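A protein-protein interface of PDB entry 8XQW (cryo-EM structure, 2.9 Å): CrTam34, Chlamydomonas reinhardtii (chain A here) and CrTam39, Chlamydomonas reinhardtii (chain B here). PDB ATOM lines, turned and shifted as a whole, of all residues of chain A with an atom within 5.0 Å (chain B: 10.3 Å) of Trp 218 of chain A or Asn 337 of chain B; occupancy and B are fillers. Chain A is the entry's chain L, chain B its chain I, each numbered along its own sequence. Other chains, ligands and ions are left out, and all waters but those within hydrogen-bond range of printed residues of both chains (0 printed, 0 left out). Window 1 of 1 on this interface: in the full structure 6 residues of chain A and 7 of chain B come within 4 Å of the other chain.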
ATOM      1  N   GLU A 214       0.087  22.563 -11.245  1.00  0.00           N
ATOM      2  CA  GLU A 214      -0.063  23.525 -10.166  1.00  0.00           C
ATOM      3  C   GLU A 214       0.031  22.880  -8.794  1.00  0.00           C
ATOM      4  O   GLU A 214       0.618  23.467  -7.875  1.00  0.00           O
ATOM      5  CB  GLU A 214      -1.386  24.250 -10.320  1.00  0.00           C
ATOM      6  CG  GLU A 214      -1.453  25.117 -11.545  1.00  0.00           C
ATOM      7  CD  GLU A 214      -0.814  26.482 -11.341  1.00  0.00           C
ATOM      8  OE1 GLU A 214      -1.514  27.406 -10.875  1.00  0.00           O
ATOM      9  OE2 GLU A 214       0.385  26.638 -11.651  1.00  0.00           O
ATOM     10  N   ASN A 215      -0.528  21.682  -8.633  1.00  0.00           N
ATOM     11  CA  ASN A 215      -0.453  20.996  -7.353  1.00  0.00           C
ATOM     12  C   ASN A 215       0.981  20.629  -7.017  1.00  0.00           C
ATOM     13  O   ASN A 215       1.427  20.799  -5.883  1.00  0.00           O
ATOM     14  CB  ASN A 215      -1.316  19.749  -7.375  1.00  0.00           C
ATOM     15  CG  ASN A 215      -2.747  20.042  -7.654  1.00  0.00           C
ATOM     16  OD1 ASN A 215      -3.508  20.358  -6.761  1.00  0.00           O
ATOM     17  ND2 ASN A 215      -3.130  19.929  -8.903  1.00  0.00           N
ATOM     18  N   GLU A 216       1.718  20.114  -7.990  1.00  0.00           N
ATOM     19  CA  GLU A 216       3.091  19.724  -7.725  1.00  0.00           C
ATOM     20  C   GLU A 216       3.975  20.930  -7.498  1.00  0.00           C
ATOM     21  O   GLU A 216       4.920  20.868  -6.712  1.00  0.00           O
ATOM     22  CB  GLU A 216       3.614  18.885  -8.875  1.00  0.00           C
ATOM     23  CG  GLU A 216       2.828  17.637  -9.096  1.00  0.00           C
ATOM     24  CD  GLU A 216       1.653  17.843 -10.000  1.00  0.00           C
ATOM     25  OE1 GLU A 216       1.365  18.998 -10.313  1.00  0.00           O
ATOM     26  OE2 GLU A 216       1.016  16.862 -10.411  1.00  0.00           O
ATOM     27  N   ARG A 217       3.686  22.033  -8.164  1.00  0.00           N
ATOM     28  CA  ARG A 217       4.451  23.246  -7.940  1.00  0.00           C
ATOM     29  C   ARG A 217       4.262  23.741  -6.519  1.00  0.00           C
ATOM     30  O   ARG A 217       5.232  24.069  -5.835  1.00  0.00           O
ATOM     31  CB  ARG A 217       4.024  24.298  -8.946  1.00  0.00           C
ATOM     32  CG  ARG A 217       4.965  25.433  -9.138  1.00  0.00           C
ATOM     33  CD  ARG A 217       4.333  26.421 -10.061  1.00  0.00           C
ATOM     34  NE  ARG A 217       4.999  27.710 -10.030  1.00  0.00           N
ATOM     35  CZ  ARG A 217       4.518  28.802 -10.605  1.00  0.00           C
ATOM     36  NH1 ARG A 217       3.371  28.750 -11.250  1.00  0.00           N
ATOM     37  NH2 ARG A 217       5.181  29.936 -10.539  1.00  0.00           N
ATOM     38  N   TRP A 218       3.018  23.790  -6.045  1.00  0.00           N
ATOM     39  CA  TRP A 218       2.821  24.210  -4.666  1.00  0.00           C
ATOM     40  C   TRP A 218       3.435  23.227  -3.693  1.00  0.00           C
ATOM     41  O   TRP A 218       3.984  23.640  -2.676  1.00  0.00           O
ATOM     42  CB  TRP A 218       1.344  24.385  -4.363  1.00  0.00           C
ATOM     43  CG  TRP A 218       1.063  24.971  -3.029  1.00  0.00           C
ATOM     44  CD1 TRP A 218       1.027  26.276  -2.713  1.00  0.00           C
ATOM     45  CD2 TRP A 218       0.756  24.262  -1.833  1.00  0.00           C
ATOM     46  NE1 TRP A 218       0.724  26.437  -1.398  1.00  0.00           N
ATOM     47  CE2 TRP A 218       0.549  25.206  -0.837  1.00  0.00           C
ATOM     48  CE3 TRP A 218       0.639  22.916  -1.511  1.00  0.00           C
ATOM     49  CZ2 TRP A 218       0.240  24.854   0.455  1.00  0.00           C
ATOM     50  CZ3 TRP A 218       0.326  22.573  -0.241  1.00  0.00           C
ATOM     51  CH2 TRP A 218       0.131  23.531   0.729  1.00  0.00           C
ATOM     52  N   PHE A 219       3.374  21.932  -3.982  1.00  0.00           N
ATOM     53  CA  PHE A 219       3.964  20.964  -3.071  1.00  0.00           C
ATOM     54  C   PHE A 219       5.460  21.177  -2.945  1.00  0.00           C
ATOM     55  O   PHE A 219       5.995  21.256  -1.840  1.00  0.00           O
ATOM     56  CB  PHE A 219       3.672  19.553  -3.539  1.00  0.00           C
ATOM     57  CG  PHE A 219       4.366  18.509  -2.745  1.00  0.00           C
ATOM     58  CD1 PHE A 219       3.927  18.177  -1.495  1.00  0.00           C
ATOM     59  CD2 PHE A 219       5.451  17.850  -3.248  1.00  0.00           C
ATOM     60  CE1 PHE A 219       4.567  17.226  -0.773  1.00  0.00           C
ATOM     61  CE2 PHE A 219       6.088  16.903  -2.522  1.00  0.00           C
ATOM     62  CZ  PHE A 219       5.643  16.586  -1.291  1.00  0.00           C
ATOM     63  N   TRP A 220       6.157  21.287  -4.064  1.00  0.00           N
ATOM     64  CA  TRP A 220       7.598  21.438  -3.988  1.00  0.00           C
ATOM     65  C   TRP A 220       8.029  22.819  -3.539  1.00  0.00           C
ATOM     66  O   TRP A 220       9.171  22.975  -3.115  1.00  0.00           O
ATOM     67  CB  TRP A 220       8.231  21.109  -5.332  1.00  0.00           C
ATOM     68  CG  TRP A 220       8.313  19.660  -5.577  1.00  0.00           C
ATOM     69  CD1 TRP A 220       7.662  18.966  -6.528  1.00  0.00           C
ATOM     70  CD2 TRP A 220       9.082  18.711  -4.846  1.00  0.00           C
ATOM     71  NE1 TRP A 220       7.969  17.643  -6.443  1.00  0.00           N
ATOM     72  CE2 TRP A 220       8.844  17.461  -5.412  1.00  0.00           C
ATOM     73  CE3 TRP A 220       9.949  18.800  -3.759  1.00  0.00           C
ATOM     74  CZ2 TRP A 220       9.441  16.313  -4.938  1.00  0.00           C
ATOM     75  CZ3 TRP A 220      10.536  17.667  -3.297  1.00  0.00           C
ATOM     76  CH2 TRP A 220      10.279  16.438  -3.879  1.00  0.00           C
ATOM     77  N   GLU A 221       7.163  23.822  -3.594  1.00  0.00           N
ATOM     78  CA  GLU A 221       7.597  25.149  -3.182  1.00  0.00           C
ATOM     79  C   GLU A 221       7.222  25.503  -1.756  1.00  0.00           C
ATOM     80  O   GLU A 221       7.952  26.257  -1.114  1.00  0.00           O
ATOM     81  CB  GLU A 221       7.019  26.213  -4.105  1.00  0.00           C
ATOM     82  CG  GLU A 221       7.517  26.141  -5.516  1.00  0.00           C
ATOM     83  CD  GLU A 221       8.841  26.826  -5.693  1.00  0.00           C
ATOM     84  OE1 GLU A 221       9.125  27.764  -4.925  1.00  0.00           O
ATOM     85  OE2 GLU A 221       9.601  26.428  -6.597  1.00  0.00           O
ATOM     86  N   VAL A 222       6.110  24.999  -1.235  1.00  0.00           N
ATOM     87  CA  VAL A 222       5.591  25.506   0.027  1.00  0.00           C
ATOM     88  C   VAL A 222       5.441  24.404   1.064  1.00  0.00           C
ATOM     89  O   VAL A 222       5.408  24.670   2.266  1.00  0.00           O
ATOM     90  CB  VAL A 222       4.257  26.226  -0.212  1.00  0.00           C
ATOM     91  CG1 VAL A 222       3.689  26.726   1.065  1.00  0.00           C
ATOM     92  CG2 VAL A 222       4.463  27.382  -1.136  1.00  0.00           C
ATOM     93  N   PHE A 223       5.381  23.160   0.632  1.00  0.00           N
ATOM     94  CA  PHE A 223       5.015  22.090   1.542  1.00  0.00           C
ATOM     95  C   PHE A 223       6.107  21.070   1.790  1.00  0.00           C
ATOM     96  O   PHE A 223       6.136  20.479   2.856  1.00  0.00           O
ATOM     97  CB  PHE A 223       3.784  21.371   1.010  1.00  0.00           C
ATOM     98  CG  PHE A 223       3.139  20.474   1.996  1.00  0.00           C
ATOM     99  CD1 PHE A 223       2.233  20.964   2.889  1.00  0.00           C
ATOM    100  CD2 PHE A 223       3.420  19.137   2.015  1.00  0.00           C
ATOM    101  CE1 PHE A 223       1.644  20.141   3.789  1.00  0.00           C
ATOM    102  CE2 PHE A 223       2.829  18.320   2.914  1.00  0.00           C
ATOM    103  CZ  PHE A 223       1.939  18.818   3.796  1.00  0.00           C
ATOM    104  N   ALA B 333      -7.419  10.719  -6.408  1.00  0.00           N
ATOM    105  CA  ALA B 333      -6.075  11.250  -6.482  1.00  0.00           C
ATOM    106  C   ALA B 333      -5.769  11.928  -5.158  1.00  0.00           C
ATOM    107  O   ALA B 333      -6.535  11.822  -4.201  1.00  0.00           O
ATOM    108  CB  ALA B 333      -5.948  12.196  -7.676  1.00  0.00           C
ATOM    109  N   LEU B 334      -4.674  12.604  -5.098  1.00  0.00           N
ATOM    110  CA  LEU B 334      -4.448  13.363  -3.891  1.00  0.00           C
ATOM    111  C   LEU B 334      -5.260  14.653  -3.946  1.00  0.00           C
ATOM    112  O   LEU B 334      -5.469  15.213  -5.021  1.00  0.00           O
ATOM    113  CB  LEU B 334      -2.971  13.664  -3.730  1.00  0.00           C
ATOM    114  CG  LEU B 334      -2.029  12.473  -3.825  1.00  0.00           C
ATOM    115  CD1 LEU B 334      -0.653  12.922  -4.115  1.00  0.00           C
ATOM    116  CD2 LEU B 334      -2.026  11.727  -2.549  1.00  0.00           C
ATOM    117  N   PRO B 335      -5.753  15.133  -2.807  1.00  0.00           N
ATOM    118  CA  PRO B 335      -6.719  16.221  -2.835  1.00  0.00           C
ATOM    119  C   PRO B 335      -6.086  17.500  -3.344  1.00  0.00           C
ATOM    120  O   PRO B 335      -4.853  17.649  -3.331  1.00  0.00           O
ATOM    121  CB  PRO B 335      -7.144  16.347  -1.370  1.00  0.00           C
ATOM    122  CG  PRO B 335      -6.069  15.731  -0.627  1.00  0.00           C
ATOM    123  CD  PRO B 335      -5.566  14.623  -1.445  1.00  0.00           C
ATOM    124  N   PRO B 336      -6.893  18.451  -3.801  1.00  0.00           N
ATOM    125  CA  PRO B 336      -6.337  19.675  -4.382  1.00  0.00           C
ATOM    126  C   PRO B 336      -5.613  20.533  -3.363  1.00  0.00           C
ATOM    127  O   PRO B 336      -5.964  20.564  -2.187  1.00  0.00           O
ATOM    128  CB  PRO B 336      -7.574  20.389  -4.922  1.00  0.00           C
ATOM    129  CG  PRO B 336      -8.525  19.320  -5.159  1.00  0.00           C
ATOM    130  CD  PRO B 336      -8.327  18.335  -4.076  1.00  0.00           C
ATOM    131  N   ASN B 337      -4.601  21.238  -3.841  1.00  0.00           N
ATOM    132  CA  ASN B 337      -3.776  22.121  -3.041  1.00  0.00           C
ATOM    133  C   ASN B 337      -4.404  23.488  -2.929  1.00  0.00           C
ATOM    134  O   ASN B 337      -5.354  23.805  -3.627  1.00  0.00           O
ATOM    135  CB  ASN B 337      -2.424  22.310  -3.700  1.00  0.00           C
ATOM    136  CG  ASN B 337      -1.511  21.215  -3.426  1.00  0.00           C
ATOM    137  OD1 ASN B 337      -0.516  21.051  -4.103  1.00  0.00           O
ATOM    138  ND2 ASN B 337      -1.819  20.446  -2.421  1.00  0.00           N
ATOM    139  N   PRO B 338      -3.868  24.340  -2.062  1.00  0.00           N
ATOM    140  CA  PRO B 338      -4.075  25.774  -2.233  1.00  0.00           C
ATOM    141  C   PRO B 338      -3.354  26.342  -3.426  1.00  0.00           C
ATOM    142  O   PRO B 338      -3.454  27.546  -3.665  1.00  0.00           O
ATOM    143  CB  PRO B 338      -3.517  26.357  -0.943  1.00  0.00           C
ATOM    144  CG  PRO B 338      -3.607  25.303   0.001  1.00  0.00           C
ATOM    145  CD  PRO B 338      -3.389  24.038  -0.715  1.00  0.00           C
ATOM    146  N   GLY B 339      -2.626  25.534  -4.171  1.00  0.00           N
ATOM    147  CA  GLY B 339      -1.888  26.033  -5.301  1.00  0.00           C
ATOM    148  C   GLY B 339      -2.692  25.854  -6.557  1.00  0.00           C
ATOM    149  O   GLY B 339      -2.513  26.585  -7.526  1.00  0.00           O
ATOM    150  N   ALA B 340      -3.590  24.885  -6.551  1.00  0.00           N
ATOM    151  CA  ALA B 340      -4.462  24.663  -7.686  1.00  0.00           C
ATOM    152  C   ALA B 340      -5.615  25.646  -7.745  1.00  0.00           C
ATOM    153  O   ALA B 340      -6.083  25.963  -8.838  1.00  0.00           O
ATOM    154  CB  ALA B 340      -5.021  23.249  -7.646  1.00  0.00           C
ATOM    155  N   VAL B 341      -6.075  26.146  -6.602  1.00  0.00           N
ATOM    156  CA  VAL B 341      -7.217  27.038  -6.534  1.00  0.00           C
ATOM    157  C   VAL B 341      -6.802  28.490  -6.401  1.00  0.00           C
ATOM    158  O   VAL B 341      -7.630  29.325  -6.058  1.00  0.00           O
ATOM    159  CB  VAL B 341      -8.160  26.650  -5.391  1.00  0.00           C
ATOM    160  CG1 VAL B 341      -8.653  25.265  -5.573  1.00  0.00           C
ATOM    161  CG2 VAL B 341      -7.462  26.785  -4.084  1.00  0.00           C
ATOM    162  N   PHE B 342      -5.542  28.823  -6.652  1.00  0.00           N
ATOM    163  CA  PHE B 342      -5.160  30.226  -6.572  1.00  0.00           C
ATOM    164  C   PHE B 342      -5.871  31.040  -7.633  1.00  0.00           C
ATOM    165  O   PHE B 342      -6.322  32.156  -7.369  1.00  0.00           O
ATOM    166  CB  PHE B 342      -3.653  30.388  -6.710  1.00  0.00           C
ATOM    167  CG  PHE B 342      -3.203  31.817  -6.777  1.00  0.00           C
ATOM    168  CD1 PHE B 342      -3.353  32.655  -5.703  1.00  0.00           C
ATOM    169  CD2 PHE B 342      -2.631  32.324  -7.914  1.00  0.00           C
ATOM    170  CE1 PHE B 342      -2.944  33.952  -5.771  1.00  0.00           C
ATOM    171  CE2 PHE B 342      -2.219  33.621  -7.970  1.00  0.00           C
ATOM    172  CZ  PHE B 342      -2.383  34.431  -6.907  1.00  0.00           C
ATOM    173  N   LYS B 343      -5.990  30.499  -8.837  1.00  0.00           N
ATOM    174  CA  LYS B 343      -6.603  31.207  -9.955  1.00  0.00           C
ATOM    175  C   LYS B 343      -7.996  30.696 -10.261  1.00  0.00           C
ATOM    176  O   LYS B 343      -8.496  30.907 -11.361  1.00  0.00           O
ATOM    177  CB  LYS B 343      -5.724  31.090 -11.188  1.00  0.00           C
ATOM    178  CG  LYS B 343      -4.412  31.799 -11.085  1.00  0.00           C
ATOM    179  CD  LYS B 343      -3.505  31.374 -12.197  1.00  0.00           C
ATOM    180  CE  LYS B 343      -2.352  32.319 -12.327  1.00  0.00           C
ATOM    181  NZ  LYS B 343      -1.130  31.627 -12.791  1.00  0.00           N
ATOM    182  N   SER B 344      -8.644  30.041  -9.341  1.00  0.00           N
ATOM    183  CA  SER B 344      -9.949  29.528  -9.715  1.00  0.00           C
ATOM    184  C   SER B 344     -11.001  30.622  -9.572  1.00  0.00           C
ATOM    185  O   SER B 344     -10.848  31.524  -8.747  1.00  0.00           O
ATOM    186  CB  SER B 344     -10.329  28.331  -8.859  1.00  0.00           C
ATOM    187  OG  SER B 344     -11.036  28.746  -7.713  1.00  0.00           O
ATOM    188  N   TYR B 349     -15.304  27.655  -3.205  1.00  0.00           N
ATOM    189  CA  TYR B 349     -14.423  26.505  -3.342  1.00  0.00           C
ATOM    190  C   TYR B 349     -13.037  26.804  -2.801  1.00  0.00           C
ATOM    191  O   TYR B 349     -12.450  25.986  -2.081  1.00  0.00           O
ATOM    192  CB  TYR B 349     -14.349  26.093  -4.804  1.00  0.00           C
ATOM    193  CG  TYR B 349     -13.642  24.797  -5.030  1.00  0.00           C
ATOM    194  CD1 TYR B 349     -13.978  23.678  -4.310  1.00  0.00           C
ATOM    195  CD2 TYR B 349     -12.643  24.690  -5.969  1.00  0.00           C
ATOM    196  CE1 TYR B 349     -13.333  22.496  -4.509  1.00  0.00           C
ATOM    197  CE2 TYR B 349     -11.997  23.513  -6.174  1.00  0.00           C
ATOM    198  CZ  TYR B 349     -12.347  22.420  -5.443  1.00  0.00           C
ATOM    199  OH  TYR B 349     -11.700  21.234  -5.642  1.00  0.00           O
ATOM    200  N   ARG B 350     -12.498  27.968  -3.138  1.00  0.00           N
ATOM    201  CA  ARG B 350     -11.187  28.337  -2.638  1.00  0.00           C
ATOM    202  C   ARG B 350     -11.175  28.404  -1.124  1.00  0.00           C
ATOM    203  O   ARG B 350     -10.231  27.936  -0.483  1.00  0.00           O
ATOM    204  CB  ARG B 350     -10.767  29.669  -3.220  1.00  0.00           C
ATOM    205  CG  ARG B 350      -9.452  30.091  -2.698  1.00  0.00           C
ATOM    206  CD  ARG B 350      -9.064  31.422  -3.208  1.00  0.00           C
ATOM    207  NE  ARG B 350      -9.748  31.734  -4.439  1.00  0.00           N
ATOM    208  CZ  ARG B 350      -9.305  32.634  -5.296  1.00  0.00           C
ATOM    209  NH1 ARG B 350      -8.178  33.275  -5.035  1.00  0.00           N
ATOM    210  NH2 ARG B 350      -9.976  32.890  -6.406  1.00  0.00           N
ATOM    211  N   ALA B 351     -12.210  28.990  -0.534  1.00  0.00           N
ATOM    212  CA  ALA B 351     -12.292  29.038   0.916  1.00  0.00           C
ATOM    213  C   ALA B 351     -12.325  27.643   1.510  1.00  0.00           C
ATOM    214  O   ALA B 351     -11.677  27.381   2.524  1.00  0.00           O
ATOM    215  CB  ALA B 351     -13.527  29.819   1.334  1.00  0.00           C
ATOM    216  N   SER B 352     -13.074  26.734   0.895  1.00  0.00           N
ATOM    217  CA  SER B 352     -13.147  25.373   1.414  1.00  0.00           C
ATOM    218  C   SER B 352     -11.779  24.708   1.422  1.00  0.00           C
ATOM    219  O   SER B 352     -11.382  24.072   2.408  1.00  0.00           O
ATOM    220  CB  SER B 352     -14.126  24.565   0.577  1.00  0.00           C
ATOM    221  OG  SER B 352     -13.710  23.225   0.490  1.00  0.00           O
ATOM    222  N   VAL B 353     -11.036  24.844   0.327  1.00  0.00           N
ATOM    223  CA  VAL B 353      -9.733  24.187   0.232  1.00  0.00           C
ATOM    224  C   VAL B 353      -8.753  24.789   1.230  1.00  0.00           C
ATOM    225  O   VAL B 353      -8.038  24.068   1.938  1.00  0.00           O
ATOM    226  CB  VAL B 353      -9.197  24.268  -1.203  1.00  0.00           C
ATOM    227  CG1 VAL B 353      -7.755  23.965  -1.221  1.00  0.00           C
ATOM    228  CG2 VAL B 353      -9.907  23.289  -2.055  1.00  0.00           C
ATOM    229  N   TRP B 354      -8.697  26.118   1.302  1.00  0.00           N
ATOM    230  CA  TRP B 354      -7.836  26.763   2.281  1.00  0.00           C
ATOM    231  C   TRP B 354      -8.163  26.297   3.685  1.00  0.00           C
ATOM    232  O   TRP B 354      -7.268  26.062   4.494  1.00  0.00           O
ATOM    233  CB  TRP B 354      -7.980  28.270   2.205  1.00  0.00           C
ATOM    234  CG  TRP B 354      -7.356  28.895   1.055  1.00  0.00           C
ATOM    235  CD1 TRP B 354      -6.920  28.291  -0.066  1.00  0.00           C
ATOM    236  CD2 TRP B 354      -7.110  30.280   0.893  1.00  0.00           C
ATOM    237  NE1 TRP B 354      -6.405  29.215  -0.930  1.00  0.00           N
ATOM    238  CE2 TRP B 354      -6.507  30.450  -0.354  1.00  0.00           C
ATOM    239  CE3 TRP B 354      -7.328  31.397   1.690  1.00  0.00           C
ATOM    240  CZ2 TRP B 354      -6.132  31.692  -0.830  1.00  0.00           C
ATOM    241  CZ3 TRP B 354      -6.953  32.620   1.218  1.00  0.00           C
ATOM    242  CH2 TRP B 354      -6.361  32.762  -0.022  1.00  0.00           C
ATOM    243  N   GLN B 355      -9.447  26.183   4.002  1.00  0.00           N
ATOM    244  CA  GLN B 355      -9.846  25.714   5.321  1.00  0.00           C
ATOM    245  C   GLN B 355      -9.292  24.334   5.603  1.00  0.00           C
ATOM    246  O   GLN B 355      -8.738  24.084   6.675  1.00  0.00           O
ATOM    247  CB  GLN B 355     -11.363  25.701   5.422  1.00  0.00           C
ATOM    248  CG  GLN B 355     -11.891  24.857   6.543  1.00  0.00           C
ATOM    249  CD  GLN B 355     -11.717  25.505   7.886  1.00  0.00           C
ATOM    250  OE1 GLN B 355     -11.638  24.827   8.907  1.00  0.00           O
ATOM    251  NE2 GLN B 355     -11.660  26.828   7.899  1.00  0.00           N
ATOM    252  N   LYS B 356      -9.439  23.416   4.650  1.00  0.00           N
ATOM    253  CA  LYS B 356      -8.984  22.051   4.887  1.00  0.00           C
ATOM    254  C   LYS B 356      -7.483  21.975   5.074  1.00  0.00           C
ATOM    255  O   LYS B 356      -7.001  21.157   5.856  1.00  0.00           O
ATOM    256  CB  LYS B 356      -9.402  21.156   3.740  1.00  0.00           C
ATOM    257  CG  LYS B 356     -10.771  20.610   3.893  1.00  0.00           C
ATOM    258  CD  LYS B 356     -11.246  20.052   2.586  1.00  0.00           C
ATOM    259  CE  LYS B 356     -12.613  19.451   2.721  1.00  0.00           C
ATOM    260  NZ  LYS B 356     -13.015  18.764   1.476  1.00  0.00           N
ATOM    261  N   TRP B 357      -6.725  22.792   4.364  1.00  0.00           N
ATOM    262  CA  TRP B 357      -5.277  22.681   4.447  1.00  0.00           C
ATOM    263  C   TRP B 357      -4.675  23.456   5.607  1.00  0.00           C
ATOM    264  O   TRP B 357      -3.466  23.388   5.807  1.00  0.00           O
ATOM    265  CB  TRP B 357      -4.640  23.126   3.136  1.00  0.00           C
ATOM    266  CG  TRP B 357      -4.643  22.047   2.141  1.00  0.00           C
ATOM    267  CD1 TRP B 357      -5.593  21.802   1.214  1.00  0.00           C
ATOM    268  CD2 TRP B 357      -3.666  21.031   1.990  1.00  0.00           C
ATOM    269  NE1 TRP B 357      -5.266  20.703   0.483  1.00  0.00           N
ATOM    270  CE2 TRP B 357      -4.079  20.210   0.943  1.00  0.00           C
ATOM    271  CE3 TRP B 357      -2.473  20.738   2.637  1.00  0.00           C
ATOM    272  CZ2 TRP B 357      -3.348  19.121   0.529  1.00  0.00           C
ATOM    273  CZ3 TRP B 357      -1.752  19.664   2.221  1.00  0.00           C
ATOM    274  CH2 TRP B 357      -2.189  18.866   1.180  1.00  0.00           C
ATOM    275  N   GLY B 358      -5.469  24.176   6.377  1.00  0.00           N
ATOM    276  CA  GLY B 358      -4.972  24.847   7.551  1.00  0.00           C
ATOM    277  C   GLY B 358      -4.796  26.339   7.441  1.00  0.00           C
ATOM    278  O   GLY B 358      -4.159  26.928   8.312  1.00  0.00           O
ATOM    279  N   TYR B 359      -5.337  26.972   6.406  1.00  0.00           N
ATOM    280  CA  TYR B 359      -5.190  28.403   6.194  1.00  0.00           C
ATOM    281  C   TYR B 359      -6.517  29.136   6.304  1.00  0.00           C
ATOM    282  O   TYR B 359      -6.740  30.119   5.603  1.00  0.00           O
ATOM    283  CB  TYR B 359      -4.573  28.687   4.834  1.00  0.00           C
ATOM    284  CG  TYR B 359      -3.234  28.062   4.640  1.00  0.00           C
ATOM    285  CD1 TYR B 359      -2.101  28.660   5.130  1.00  0.00           C
ATOM    286  CD2 TYR B 359      -3.103  26.869   3.968  1.00  0.00           C
ATOM    287  CE1 TYR B 359      -0.887  28.093   4.960  1.00  0.00           C
ATOM    288  CE2 TYR B 359      -1.888  26.295   3.801  1.00  0.00           C
ATOM    289  CZ  TYR B 359      -0.787  26.912   4.298  1.00  0.00           C
ATOM    290  OH  TYR B 359       0.438  26.341   4.124  1.00  0.00           O
ATOM    291  N   VAL B 362      -6.342  33.099   6.882  1.00  0.00           N
ATOM    292  CA  VAL B 362      -5.688  34.025   5.976  1.00  0.00           C
ATOM    293  C   VAL B 362      -6.735  34.901   5.303  1.00  0.00           C
ATOM    294  O   VAL B 362      -7.891  34.507   5.122  1.00  0.00           O
ATOM    295  CB  VAL B 362      -4.844  33.249   4.954  1.00  0.00           C
ATOM    296  CG1 VAL B 362      -4.013  34.173   4.126  1.00  0.00           C
ATOM    297  CG2 VAL B 362      -3.949  32.293   5.672  1.00  0.00           C
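The guanidinium group (NH1) of Arg 217 of chain A is in salt-bridge range of the side-chain carboxylate (OE2) of Glu 214 of chain A, 3.7 Å away.
O of Pro 336 of chain B sits at hydrogen-bond distance from NE1 of Trp 357 of chain B (2.8 Å).
N of Tyr 359 of chain B lies within hydrogen-bond range of O of Trp 354 of chain B.
Trp 218 of chain A touches just these residues of chain B: Asn 337, Pro 338, Gly 339 and Tyr 359.
Of the printed residues of chain B, Asn 215 of chain A touches Pro 336 (3.8 Å), Asn 337 (2.6 Å) and Ala 340 (3.4 Å).
No residue of chain B comes within 4 Å of Val 222 of chain A.
Printed residues of chain B within 4 Å of Phe 223 of chain A: Trp 357 (3.8 Å).
Of the printed residues of chain A, Trp 357 of chain B touches Phe 223.
The backbone carbonyl oxygen of Asn 215 of chain A sits close to the side-chain amide oxygen of Asn 337 of chain B.
Among the printed residues, merely in contact across the chains: Trp 218 of chain A with Asn 337 of chain B, Asn 215 of chain A with Ala 340 of chain B, Glu 214 of chain A with Gly 339 of chain B, Trp 218 of chain A with Gly 339 of chain B, Asn 215 of chain A with Pro 336 of chain B, Phe 223 of chain A with Trp 357 of chain B, Trp 218 of chain A with Pro 338 of chain B, Trp 218 of chain A with Tyr 359 of chain B and Phe 219 of chain A with Asn 337 of chain B.
Printed residues of chain B that touch a printed residue of chain A: Pro 336, Asn 337, Pro 338, Gly 339, Ala 340, Trp 357 and Tyr 359.
Hydrophobic or aromatic side chains of chain A within 4 Å of the printed part of chain B: Trp 218 and Phe 223.
Among the printed residues, 10 pairs touch across the chains.
Among the printed residues, no Asp or Glu carboxylate lies within 4 Å of a Lys or Arg side-chain nitrogen of the other chain.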
